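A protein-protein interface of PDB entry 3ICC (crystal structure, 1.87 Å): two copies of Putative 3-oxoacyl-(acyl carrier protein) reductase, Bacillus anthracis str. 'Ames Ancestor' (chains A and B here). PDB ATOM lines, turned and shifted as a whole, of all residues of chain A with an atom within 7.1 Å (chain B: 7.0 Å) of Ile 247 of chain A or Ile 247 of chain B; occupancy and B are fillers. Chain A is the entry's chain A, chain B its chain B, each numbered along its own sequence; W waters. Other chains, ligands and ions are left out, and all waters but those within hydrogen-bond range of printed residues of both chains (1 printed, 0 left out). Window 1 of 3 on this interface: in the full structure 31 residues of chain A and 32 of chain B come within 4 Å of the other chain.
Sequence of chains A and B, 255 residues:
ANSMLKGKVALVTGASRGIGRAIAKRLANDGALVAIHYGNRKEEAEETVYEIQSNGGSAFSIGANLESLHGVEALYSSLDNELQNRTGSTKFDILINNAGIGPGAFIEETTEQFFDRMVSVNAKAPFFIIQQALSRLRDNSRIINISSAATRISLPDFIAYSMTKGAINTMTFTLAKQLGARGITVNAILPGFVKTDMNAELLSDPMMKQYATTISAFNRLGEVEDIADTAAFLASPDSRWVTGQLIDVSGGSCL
Thr 230 of chain A touches Phe 233 of chain B, and with the chains exchanged Phe 233 of chain A touches Thr 230 of chain B.
Phe 233 of chain A touches its own counterpart, Phe 233 of chain B.
Val 242 of chain A touches Asp 248 of chain B, and with the chains exchanged Asp 248 of chain A touches Val 242 of chain B.
Gln 245 of chain A touches Asp 248 of chain B, and with the chains exchanged Asp 248 of chain A touches Gln 245 of chain B.
Positions printed for both chains: 187, 188, 189, 190, 191, 230, 233, 234, 242, 245, 246, 247, 248, 249 and 250.
The backbone NH of Ala 188 of chain A sits at hydrogen-bond distance from the backbone carbonyl oxygen of Gln 245 of chain A (2.9 Å).
N of Ile 247 of chain A is in hydrogen-bond range of O of Ala 188 of chain A.
N of Leu 190 of chain A sits at hydrogen-bond distance from O of Ile 247 of chain A (2.9 Å).
OD2 of Asp 248 of chain A sits at hydrogen-bond distance from OG of Ser 250 of chain A (2.4 Å).
The backbone carbonyl oxygen (O) of Val 242 of chain B lies within hydrogen-bond range of the side-chain amide nitrogen (ND2) of Asn 187 of chain B (3.0 Å).
N of Gln 245 of chain B is in hydrogen-bond range of OD1 of Asn 187 of chain B, 3.0 Å away.
Among the printed residues, merely in contact across the chains: Thr 230 of chain A with Phe 233 of chain B (3.5 Å), Thr 230 of chain A with Val 242 of chain B (3.4 Å), Phe 233 of chain A with Thr 230 of chain B (3.7 Å), Phe 233 of chain A with Phe 233 of chain B (3.4 Å), Val 242 of chain A with Thr 230 of chain B (3.4 Å), Val 242 of chain A with Asp 248 of chain B (3.98 Å), Gln 245 of chain A with Asp 248 of chain B (3.7 Å), Ile 247 of chain A with Ile 247 of chain B (3.9 Å), Asp 248 of chain A with Val 242 of chain B (3.9 Å) and Asp 248 of chain A with Gln 245 of chain B (3.7 Å).
Water W1 lies within hydrogen-bond range of O of Leu 246 of chain A and O of Leu 246 of chain B.
Printed residues of chain B within 4 Å of Ile 247 of chain A: Ile 247 (3.9 Å).
Printed residues of chain A within 4 Å of Ile 247 of chain B: Ile 247 (3.9 Å).
Printed residues of chain B within 4 Å of Val 242 of chain A: Thr 230 and Asp 248.
Of the printed residues of chain A, Val 242 of chain B touches Thr 230 (3.4 Å) and Asp 248 (3.9 Å).
Ser 250 of chain B touches none of the printed residues of chain A.
Leu 246 of chain B touches none of the printed residues of chain A.
Of the 15 printed residues of chain A, 6 touch a printed residue of chain B.
Printed residues of chain A that touch a printed residue of chain B: Thr 230, Phe 233, Val 242, Gln 245, Ile 247 and Asp 248.
Hydrophobic or aromatic side chains of chain A that line the printed part of chain B: Phe 233, Val 242 and Ile 247.
Hydrophobic or aromatic side chains of chain B within 4 Å of the printed part of chain A: Phe 233, Val 242 and Ile 247.
Among the printed residues, no Asp or Glu carboxylate lies within 4 Å of a Lys or Arg side-chain nitrogen of the other chain.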
ATOM      1  N   ASN A 187     -21.160 -20.900  20.893  1.00  0.00           N
ATOM      2  CA  ASN A 187     -22.369 -21.163  20.161  1.00  0.00           C
ATOM      3  C   ASN A 187     -22.830 -22.589  20.419  1.00  0.00           C
ATOM      4  O   ASN A 187     -22.060 -23.427  20.871  1.00  0.00           O
ATOM      5  CB  ASN A 187     -22.138 -20.984  18.645  1.00  0.00           C
ATOM      6  CG  ASN A 187     -21.860 -19.513  18.271  1.00  0.00           C
ATOM      7  OD1 ASN A 187     -22.736 -18.650  18.347  1.00  0.00           O
ATOM      8  ND2 ASN A 187     -20.650 -19.244  17.902  1.00  0.00           N
ATOM      9  N   ALA A 188     -24.067 -22.867  20.078  1.00  0.00           N
ATOM     10  CA  ALA A 188     -24.606 -24.207  20.205  1.00  0.00           C
ATOM     11  C   ALA A 188     -25.120 -24.692  18.869  1.00  0.00           C
ATOM     12  O   ALA A 188     -25.580 -23.898  18.072  1.00  0.00           O
ATOM     13  CB  ALA A 188     -25.751 -24.243  21.269  1.00  0.00           C
ATOM     14  N   ILE A 189     -25.035 -25.987  18.639  1.00  0.00           N
ATOM     15  CA  ILE A 189     -25.673 -26.608  17.469  1.00  0.00           C
ATOM     16  C   ILE A 189     -26.807 -27.468  18.024  1.00  0.00           C
ATOM     17  O   ILE A 189     -26.591 -28.213  18.992  1.00  0.00           O
ATOM     18  CB  ILE A 189     -24.655 -27.459  16.703  1.00  0.00           C
ATOM     19  CG1 ILE A 189     -23.661 -26.591  15.933  1.00  0.00           C
ATOM     20  CG2 ILE A 189     -25.348 -28.406  15.729  1.00  0.00           C
ATOM     21  CD1 ILE A 189     -22.448 -27.373  15.401  1.00  0.00           C
ATOM     22  N   LEU A 190     -27.986 -27.394  17.397  1.00  0.00           N
ATOM     23  CA  LEU A 190     -29.183 -28.082  17.839  1.00  0.00           C
ATOM     24  C   LEU A 190     -29.574 -29.087  16.750  1.00  0.00           C
ATOM     25  O   LEU A 190     -30.271 -28.740  15.835  1.00  0.00           O
ATOM     26  CB  LEU A 190     -30.293 -27.082  18.081  1.00  0.00           C
ATOM     27  CG  LEU A 190     -30.264 -26.273  19.406  1.00  0.00           C
ATOM     28  CD1 LEU A 190     -29.020 -25.333  19.573  1.00  0.00           C
ATOM     29  CD2 LEU A 190     -31.602 -25.521  19.502  1.00  0.00           C
ATOM     30  N   PRO A 191     -29.107 -30.335  16.867  1.00  0.00           N
ATOM     31  CA  PRO A 191     -29.468 -31.319  15.838  1.00  0.00           C
ATOM     32  C   PRO A 191     -30.886 -31.801  15.999  1.00  0.00           C
ATOM     33  O   PRO A 191     -31.404 -31.860  17.113  1.00  0.00           O
ATOM     34  CB  PRO A 191     -28.523 -32.497  16.096  1.00  0.00           C
ATOM     35  CG  PRO A 191     -27.393 -31.898  16.954  1.00  0.00           C
ATOM     36  CD  PRO A 191     -28.032 -30.805  17.745  1.00  0.00           C
ATOM     37  N   THR A 230     -21.580 -28.064   9.738  1.00  0.00           N
ATOM     38  CA  THR A 230     -21.881 -26.792  10.380  1.00  0.00           C
ATOM     39  C   THR A 230     -20.886 -26.487  11.516  1.00  0.00           C
ATOM     40  O   THR A 230     -20.458 -25.332  11.702  1.00  0.00           O
ATOM     41  CB  THR A 230     -23.341 -26.760  10.915  1.00  0.00           C
ATOM     42  OG1 THR A 230     -24.232 -26.726   9.793  1.00  0.00           O
ATOM     43  CG2 THR A 230     -23.623 -25.536  11.762  1.00  0.00           C
ATOM     44  N   PHE A 233     -17.807 -24.681  10.289  1.00  0.00           N
ATOM     45  CA  PHE A 233     -17.938 -23.240  10.084  1.00  0.00           C
ATOM     46  C   PHE A 233     -17.729 -22.536  11.457  1.00  0.00           C
ATOM     47  O   PHE A 233     -16.932 -21.619  11.592  1.00  0.00           O
ATOM     48  CB  PHE A 233     -19.292 -22.864   9.492  1.00  0.00           C
ATOM     49  CG  PHE A 233     -19.610 -21.368   9.593  1.00  0.00           C
ATOM     50  CD1 PHE A 233     -18.800 -20.443   8.972  1.00  0.00           C
ATOM     51  CD2 PHE A 233     -20.660 -20.917  10.334  1.00  0.00           C
ATOM     52  CE1 PHE A 233     -19.069 -19.079   9.093  1.00  0.00           C
ATOM     53  CE2 PHE A 233     -20.951 -19.555  10.466  1.00  0.00           C
ATOM     54  CZ  PHE A 233     -20.123 -18.638   9.856  1.00  0.00           C
ATOM     55  N   LEU A 234     -18.442 -23.030  12.459  1.00  0.00           N
ATOM     56  CA  LEU A 234     -18.365 -22.441  13.807  1.00  0.00           C
ATOM     57  C   LEU A 234     -16.988 -22.551  14.420  1.00  0.00           C
ATOM     58  O   LEU A 234     -16.625 -21.705  15.228  1.00  0.00           O
ATOM     59  CB  LEU A 234     -19.423 -23.049  14.721  1.00  0.00           C
ATOM     60  CG  LEU A 234     -20.850 -22.718  14.260  1.00  0.00           C
ATOM     61  CD1 LEU A 234     -21.894 -23.463  15.148  1.00  0.00           C
ATOM     62  CD2 LEU A 234     -21.119 -21.231  14.267  1.00  0.00           C
ATOM     63  N   VAL A 242     -20.227 -14.299  14.786  1.00  0.00           N
ATOM     64  CA  VAL A 242     -21.333 -15.117  15.263  1.00  0.00           C
ATOM     65  C   VAL A 242     -21.011 -15.681  16.636  1.00  0.00           C
ATOM     66  O   VAL A 242     -20.113 -16.499  16.770  1.00  0.00           O
ATOM     67  CB  VAL A 242     -21.577 -16.279  14.289  1.00  0.00           C
ATOM     68  CG1 VAL A 242     -22.796 -17.119  14.769  1.00  0.00           C
ATOM     69  CG2 VAL A 242     -21.719 -15.745  12.867  1.00  0.00           C
ATOM     70  N   GLN A 245     -25.205 -17.955  19.820  1.00  0.00           N
ATOM     71  CA  GLN A 245     -26.314 -18.336  18.978  1.00  0.00           C
ATOM     72  C   GLN A 245     -26.626 -19.823  19.040  1.00  0.00           C
ATOM     73  O   GLN A 245     -25.737 -20.652  19.194  1.00  0.00           O
ATOM     74  CB  GLN A 245     -26.050 -17.905  17.536  1.00  0.00           C
ATOM     75  CG  GLN A 245     -25.851 -16.380  17.367  1.00  0.00           C
ATOM     76  CD  GLN A 245     -26.894 -15.587  18.076  1.00  0.00           C
ATOM     77  OE1 GLN A 245     -28.096 -15.841  17.938  1.00  0.00           O
ATOM     78  NE2 GLN A 245     -26.462 -14.587  18.841  1.00  0.00           N
ATOM     79  N   LEU A 246     -27.911 -20.116  18.927  1.00  0.00           N
ATOM     80  CA  LEU A 246     -28.443 -21.491  18.958  1.00  0.00           C
ATOM     81  C   LEU A 246     -28.784 -21.828  17.517  1.00  0.00           C
ATOM     82  O   LEU A 246     -29.794 -21.377  16.996  1.00  0.00           O
ATOM     83  CB  LEU A 246     -29.684 -21.538  19.860  1.00  0.00           C
ATOM     84  CG  LEU A 246     -29.499 -20.971  21.306  1.00  0.00           C
ATOM     85  CD1 LEU A 246     -30.803 -21.068  22.137  1.00  0.00           C
ATOM     86  CD2 LEU A 246     -28.305 -21.577  22.084  1.00  0.00           C
ATOM     87  N   ILE A 247     -27.911 -22.544  16.831  1.00  0.00           N
ATOM     88  CA  ILE A 247     -28.052 -22.774  15.386  1.00  0.00           C
ATOM     89  C   ILE A 247     -28.736 -24.101  15.195  1.00  0.00           C
ATOM     90  O   ILE A 247     -28.204 -25.105  15.643  1.00  0.00           O
ATOM     91  CB  ILE A 247     -26.671 -22.892  14.706  1.00  0.00           C
ATOM     92  CG1 ILE A 247     -25.794 -21.686  15.049  1.00  0.00           C
ATOM     93  CG2 ILE A 247     -26.802 -23.044  13.200  1.00  0.00           C
ATOM     94  CD1 ILE A 247     -26.312 -20.422  14.525  1.00  0.00           C
ATOM     95  N   ASP A 248     -29.917 -24.081  14.576  1.00  0.00           N
ATOM     96  CA  ASP A 248     -30.683 -25.301  14.312  1.00  0.00           C
ATOM     97  C   ASP A 248     -30.030 -25.995  13.159  1.00  0.00           C
ATOM     98  O   ASP A 248     -29.735 -25.359  12.133  1.00  0.00           O
ATOM     99  CB  ASP A 248     -32.132 -25.021  13.949  1.00  0.00           C
ATOM    100  CG  ASP A 248     -32.898 -26.294  13.676  1.00  0.00           C
ATOM    101  OD1 ASP A 248     -33.315 -26.937  14.684  1.00  0.00           O
ATOM    102  OD2 ASP A 248     -32.964 -26.709  12.462  1.00  0.00           O
ATOM    103  N   VAL A 249     -29.754 -27.286  13.331  1.00  0.00           N
ATOM    104  CA  VAL A 249     -29.163 -28.087  12.270  1.00  0.00           C
ATOM    105  C   VAL A 249     -29.977 -29.365  12.221  1.00  0.00           C
ATOM    106  O   VAL A 249     -29.490 -30.442  12.584  1.00  0.00           O
ATOM    107  CB  VAL A 249     -27.678 -28.361  12.523  1.00  0.00           C
ATOM    108  CG1 VAL A 249     -27.055 -29.059  11.317  1.00  0.00           C
ATOM    109  CG2 VAL A 249     -26.880 -27.026  12.824  1.00  0.00           C
ATOM    110  N   SER A 250     -31.233 -29.197  11.836  1.00  0.00           N
ATOM    111  CA  SER A 250     -32.250 -30.226  11.873  1.00  0.00           C
ATOM    112  C   SER A 250     -32.893 -30.424  10.504  1.00  0.00           C
ATOM    113  O   SER A 250     -33.935 -31.089  10.401  1.00  0.00           O
ATOM    114  CB  SER A 250     -33.365 -29.858  12.855  1.00  0.00           C
ATOM    115  OG  SER A 250     -34.188 -28.775  12.378  1.00  0.00           O
ATOM    116  N   ASN B 187     -32.338 -18.808   4.345  1.00  0.00           N
ATOM    117  CA  ASN B 187     -31.878 -18.286   5.639  1.00  0.00           C
ATOM    118  C   ASN B 187     -31.741 -16.802   5.588  1.00  0.00           C
ATOM    119  O   ASN B 187     -31.703 -16.205   4.509  1.00  0.00           O
ATOM    120  CB  ASN B 187     -30.519 -18.862   5.990  1.00  0.00           C
ATOM    121  CG  ASN B 187     -30.583 -20.353   6.280  1.00  0.00           C
ATOM    122  OD1 ASN B 187     -31.206 -20.789   7.260  1.00  0.00           O
ATOM    123  ND2 ASN B 187     -29.931 -21.148   5.437  1.00  0.00           N
ATOM    124  N   ALA B 188     -31.632 -16.185   6.756  1.00  0.00           N
ATOM    125  CA  ALA B 188     -31.399 -14.745   6.836  1.00  0.00           C
ATOM    126  C   ALA B 188     -30.224 -14.474   7.702  1.00  0.00           C
ATOM    127  O   ALA B 188     -29.927 -15.219   8.622  1.00  0.00           O
ATOM    128  CB  ALA B 188     -32.661 -13.969   7.373  1.00  0.00           C
ATOM    129  N   ILE B 189     -29.510 -13.416   7.360  1.00  0.00           N
ATOM    130  CA  ILE B 189     -28.438 -12.880   8.175  1.00  0.00           C
ATOM    131  C   ILE B 189     -28.927 -11.539   8.782  1.00  0.00           C
ATOM    132  O   ILE B 189     -29.465 -10.650   8.079  1.00  0.00           O
ATOM    133  CB  ILE B 189     -27.166 -12.672   7.282  1.00  0.00           C
ATOM    134  CG1 ILE B 189     -26.548 -14.016   6.893  1.00  0.00           C
ATOM    135  CG2 ILE B 189     -26.150 -11.761   8.023  1.00  0.00           C
ATOM    136  CD1 ILE B 189     -25.448 -13.979   5.758  1.00  0.00           C
ATOM    137  N   LEU B 190     -28.777 -11.405  10.074  1.00  0.00           N
ATOM    138  CA  LEU B 190     -29.201 -10.184  10.823  1.00  0.00           C
ATOM    139  C   LEU B 190     -27.977  -9.440  11.307  1.00  0.00           C
ATOM    140  O   LEU B 190     -27.455  -9.731  12.398  1.00  0.00           O
ATOM    141  CB  LEU B 190     -30.077 -10.611  11.995  1.00  0.00           C
ATOM    142  CG  LEU B 190     -31.498 -11.080  11.638  1.00  0.00           C
ATOM    143  CD1 LEU B 190     -31.500 -12.325  10.645  1.00  0.00           C
ATOM    144  CD2 LEU B 190     -32.276 -11.365  12.942  1.00  0.00           C
ATOM    145  N   PRO B 191     -27.494  -8.477  10.507  1.00  0.00           N
ATOM    146  CA  PRO B 191     -26.310  -7.760  10.940  1.00  0.00           C
ATOM    147  C   PRO B 191     -26.599  -6.772  12.062  1.00  0.00           C
ATOM    148  O   PRO B 191     -27.730  -6.247  12.180  1.00  0.00           O
ATOM    149  CB  PRO B 191     -25.896  -6.954   9.708  1.00  0.00           C
ATOM    150  CG  PRO B 191     -26.558  -7.589   8.565  1.00  0.00           C
ATOM    151  CD  PRO B 191     -27.784  -8.264   9.073  1.00  0.00           C
ATOM    152  N   THR B 230     -19.901 -15.050   6.900  1.00  0.00           N
ATOM    153  CA  THR B 230     -21.075 -15.867   7.218  1.00  0.00           C
ATOM    154  C   THR B 230     -21.931 -16.224   5.989  1.00  0.00           C
ATOM    155  O   THR B 230     -22.362 -17.364   5.828  1.00  0.00           O
ATOM    156  CB  THR B 230     -21.960 -15.227   8.311  1.00  0.00           C
ATOM    157  OG1 THR B 230     -21.206 -15.128   9.528  1.00  0.00           O
ATOM    158  CG2 THR B 230     -23.236 -16.101   8.611  1.00  0.00           C
ATOM    159  N   PHE B 233     -20.583 -19.288   4.089  1.00  0.00           N
ATOM    160  CA  PHE B 233     -21.014 -20.579   4.653  1.00  0.00           C
ATOM    161  C   PHE B 233     -22.428 -20.927   4.216  1.00  0.00           C
ATOM    162  O   PHE B 233     -22.685 -22.044   3.772  1.00  0.00           O
ATOM    163  CB  PHE B 233     -20.947 -20.566   6.193  1.00  0.00           C
ATOM    164  CG  PHE B 233     -21.695 -21.742   6.849  1.00  0.00           C
ATOM    165  CD1 PHE B 233     -21.242 -23.033   6.697  1.00  0.00           C
ATOM    166  CD2 PHE B 233     -22.841 -21.530   7.616  1.00  0.00           C
ATOM    167  CE1 PHE B 233     -21.917 -24.125   7.278  1.00  0.00           C
ATOM    168  CE2 PHE B 233     -23.513 -22.621   8.213  1.00  0.00           C
ATOM    169  CZ  PHE B 233     -23.041 -23.927   8.015  1.00  0.00           C
ATOM    170  N   LEU B 234     -23.348 -19.986   4.371  1.00  0.00           N
ATOM    171  CA  LEU B 234     -24.747 -20.224   3.980  1.00  0.00           C
ATOM    172  C   LEU B 234     -24.880 -20.498   2.458  1.00  0.00           C
ATOM    173  O   LEU B 234     -25.723 -21.287   2.061  1.00  0.00           O
ATOM    174  CB  LEU B 234     -25.671 -19.082   4.431  1.00  0.00           C
ATOM    175  CG  LEU B 234     -25.766 -18.909   5.958  1.00  0.00           C
ATOM    176  CD1 LEU B 234     -26.606 -17.691   6.315  1.00  0.00           C
ATOM    177  CD2 LEU B 234     -26.353 -20.113   6.679  1.00  0.00           C
ATOM    178  N   VAL B 242     -28.977 -26.489   7.422  1.00  0.00           N
ATOM    179  CA  VAL B 242     -29.399 -25.261   8.065  1.00  0.00           C
ATOM    180  C   VAL B 242     -30.344 -24.559   7.101  1.00  0.00           C
ATOM    181  O   VAL B 242     -29.938 -24.104   6.008  1.00  0.00           O
ATOM    182  CB  VAL B 242     -28.192 -24.338   8.361  1.00  0.00           C
ATOM    183  CG1 VAL B 242     -28.623 -23.034   9.017  1.00  0.00           C
ATOM    184  CG2 VAL B 242     -27.171 -25.076   9.245  1.00  0.00           C
ATOM    185  N   GLN B 245     -33.465 -20.276   9.184  1.00  0.00           N
ATOM    186  CA  GLN B 245     -32.848 -19.726  10.369  1.00  0.00           C
ATOM    187  C   GLN B 245     -32.483 -18.267  10.211  1.00  0.00           C
ATOM    188  O   GLN B 245     -32.180 -17.792   9.101  1.00  0.00           O
ATOM    189  CB  GLN B 245     -31.626 -20.566  10.771  1.00  0.00           C
ATOM    190  CG  GLN B 245     -31.966 -22.055  11.059  1.00  0.00           C
ATOM    191  CD  GLN B 245     -33.212 -22.178  11.865  1.00  0.00           C
ATOM    192  OE1 GLN B 245     -33.355 -21.527  12.904  1.00  0.00           O
ATOM    193  NE2 GLN B 245     -34.149 -22.968  11.400  1.00  0.00           N
ATOM    194  N   LEU B 246     -32.533 -17.560  11.341  1.00  0.00           N
ATOM    195  CA  LEU B 246     -32.248 -16.101  11.386  1.00  0.00           C
ATOM    196  C   LEU B 246     -30.977 -16.028  12.139  1.00  0.00           C
ATOM    197  O   LEU B 246     -30.999 -16.189  13.331  1.00  0.00           O
ATOM    198  CB  LEU B 246     -33.350 -15.347  12.133  1.00  0.00           C
ATOM    199  CG  LEU B 246     -34.795 -15.673  11.734  1.00  0.00           C
ATOM    200  CD1 LEU B 246     -35.828 -14.874  12.669  1.00  0.00           C
ATOM    201  CD2 LEU B 246     -35.024 -15.371  10.230  1.00  0.00           C
ATOM    202  N   ILE B 247     -29.854 -15.867  11.437  1.00  0.00           N
ATOM    203  CA  ILE B 247     -28.521 -15.968  12.027  1.00  0.00           C
ATOM    204  C   ILE B 247     -28.063 -14.587  12.396  1.00  0.00           C
ATOM    205  O   ILE B 247     -27.932 -13.715  11.529  1.00  0.00           O
ATOM    206  CB  ILE B 247     -27.507 -16.548  11.033  1.00  0.00           C
ATOM    207  CG1 ILE B 247     -28.007 -17.872  10.458  1.00  0.00           C
ATOM    208  CG2 ILE B 247     -26.140 -16.722  11.700  1.00  0.00           C
ATOM    209  CD1 ILE B 247     -28.217 -18.961  11.453  1.00  0.00           C
ATOM    210  N   ASP B 248     -27.840 -14.369  13.678  1.00  0.00           N
ATOM    211  CA  ASP B 248     -27.315 -13.078  14.125  1.00  0.00           C
ATOM    212  C   ASP B 248     -25.821 -12.966  13.779  1.00  0.00           C
ATOM    213  O   ASP B 248     -25.005 -13.860  14.087  1.00  0.00           O
ATOM    214  CB  ASP B 248     -27.475 -12.945  15.619  1.00  0.00           C
ATOM    215  CG  ASP B 248     -27.003 -11.621  16.118  1.00  0.00           C
ATOM    216  OD1 ASP B 248     -27.774 -10.624  16.032  1.00  0.00           O
ATOM    217  OD2 ASP B 248     -25.844 -11.611  16.579  1.00  0.00           O
ATOM    218  N   VAL B 249     -25.491 -11.883  13.098  1.00  0.00           N
ATOM    219  CA  VAL B 249     -24.118 -11.553  12.764  1.00  0.00           C
ATOM    220  C   VAL B 249     -23.933 -10.120  13.204  1.00  0.00           C
ATOM    221  O   VAL B 249     -23.748  -9.224  12.361  1.00  0.00           O
ATOM    222  CB  VAL B 249     -23.827 -11.759  11.289  1.00  0.00           C
ATOM    223  CG1 VAL B 249     -22.332 -11.842  11.076  1.00  0.00           C
ATOM    224  CG2 VAL B 249     -24.467 -13.081  10.760  1.00  0.00           C
ATOM    225  N   SER B 250     -23.989  -9.941  14.534  1.00  0.00           N
ATOM    226  CA  SER B 250     -23.865  -8.651  15.215  1.00  0.00           C
ATOM    227  C   SER B 250     -22.699  -8.589  16.207  1.00  0.00           C
ATOM    228  O   SER B 250     -22.561  -7.604  16.943  1.00  0.00           O
ATOM    229  CB  SER B 250     -25.154  -8.364  16.009  1.00  0.00           C
ATOM    230  OG  SER B 250     -25.299  -9.248  17.165  1.00  0.00           O
HETATM  231  O   HOH W   1     -30.058 -18.909  15.118  1.00  0.00           O
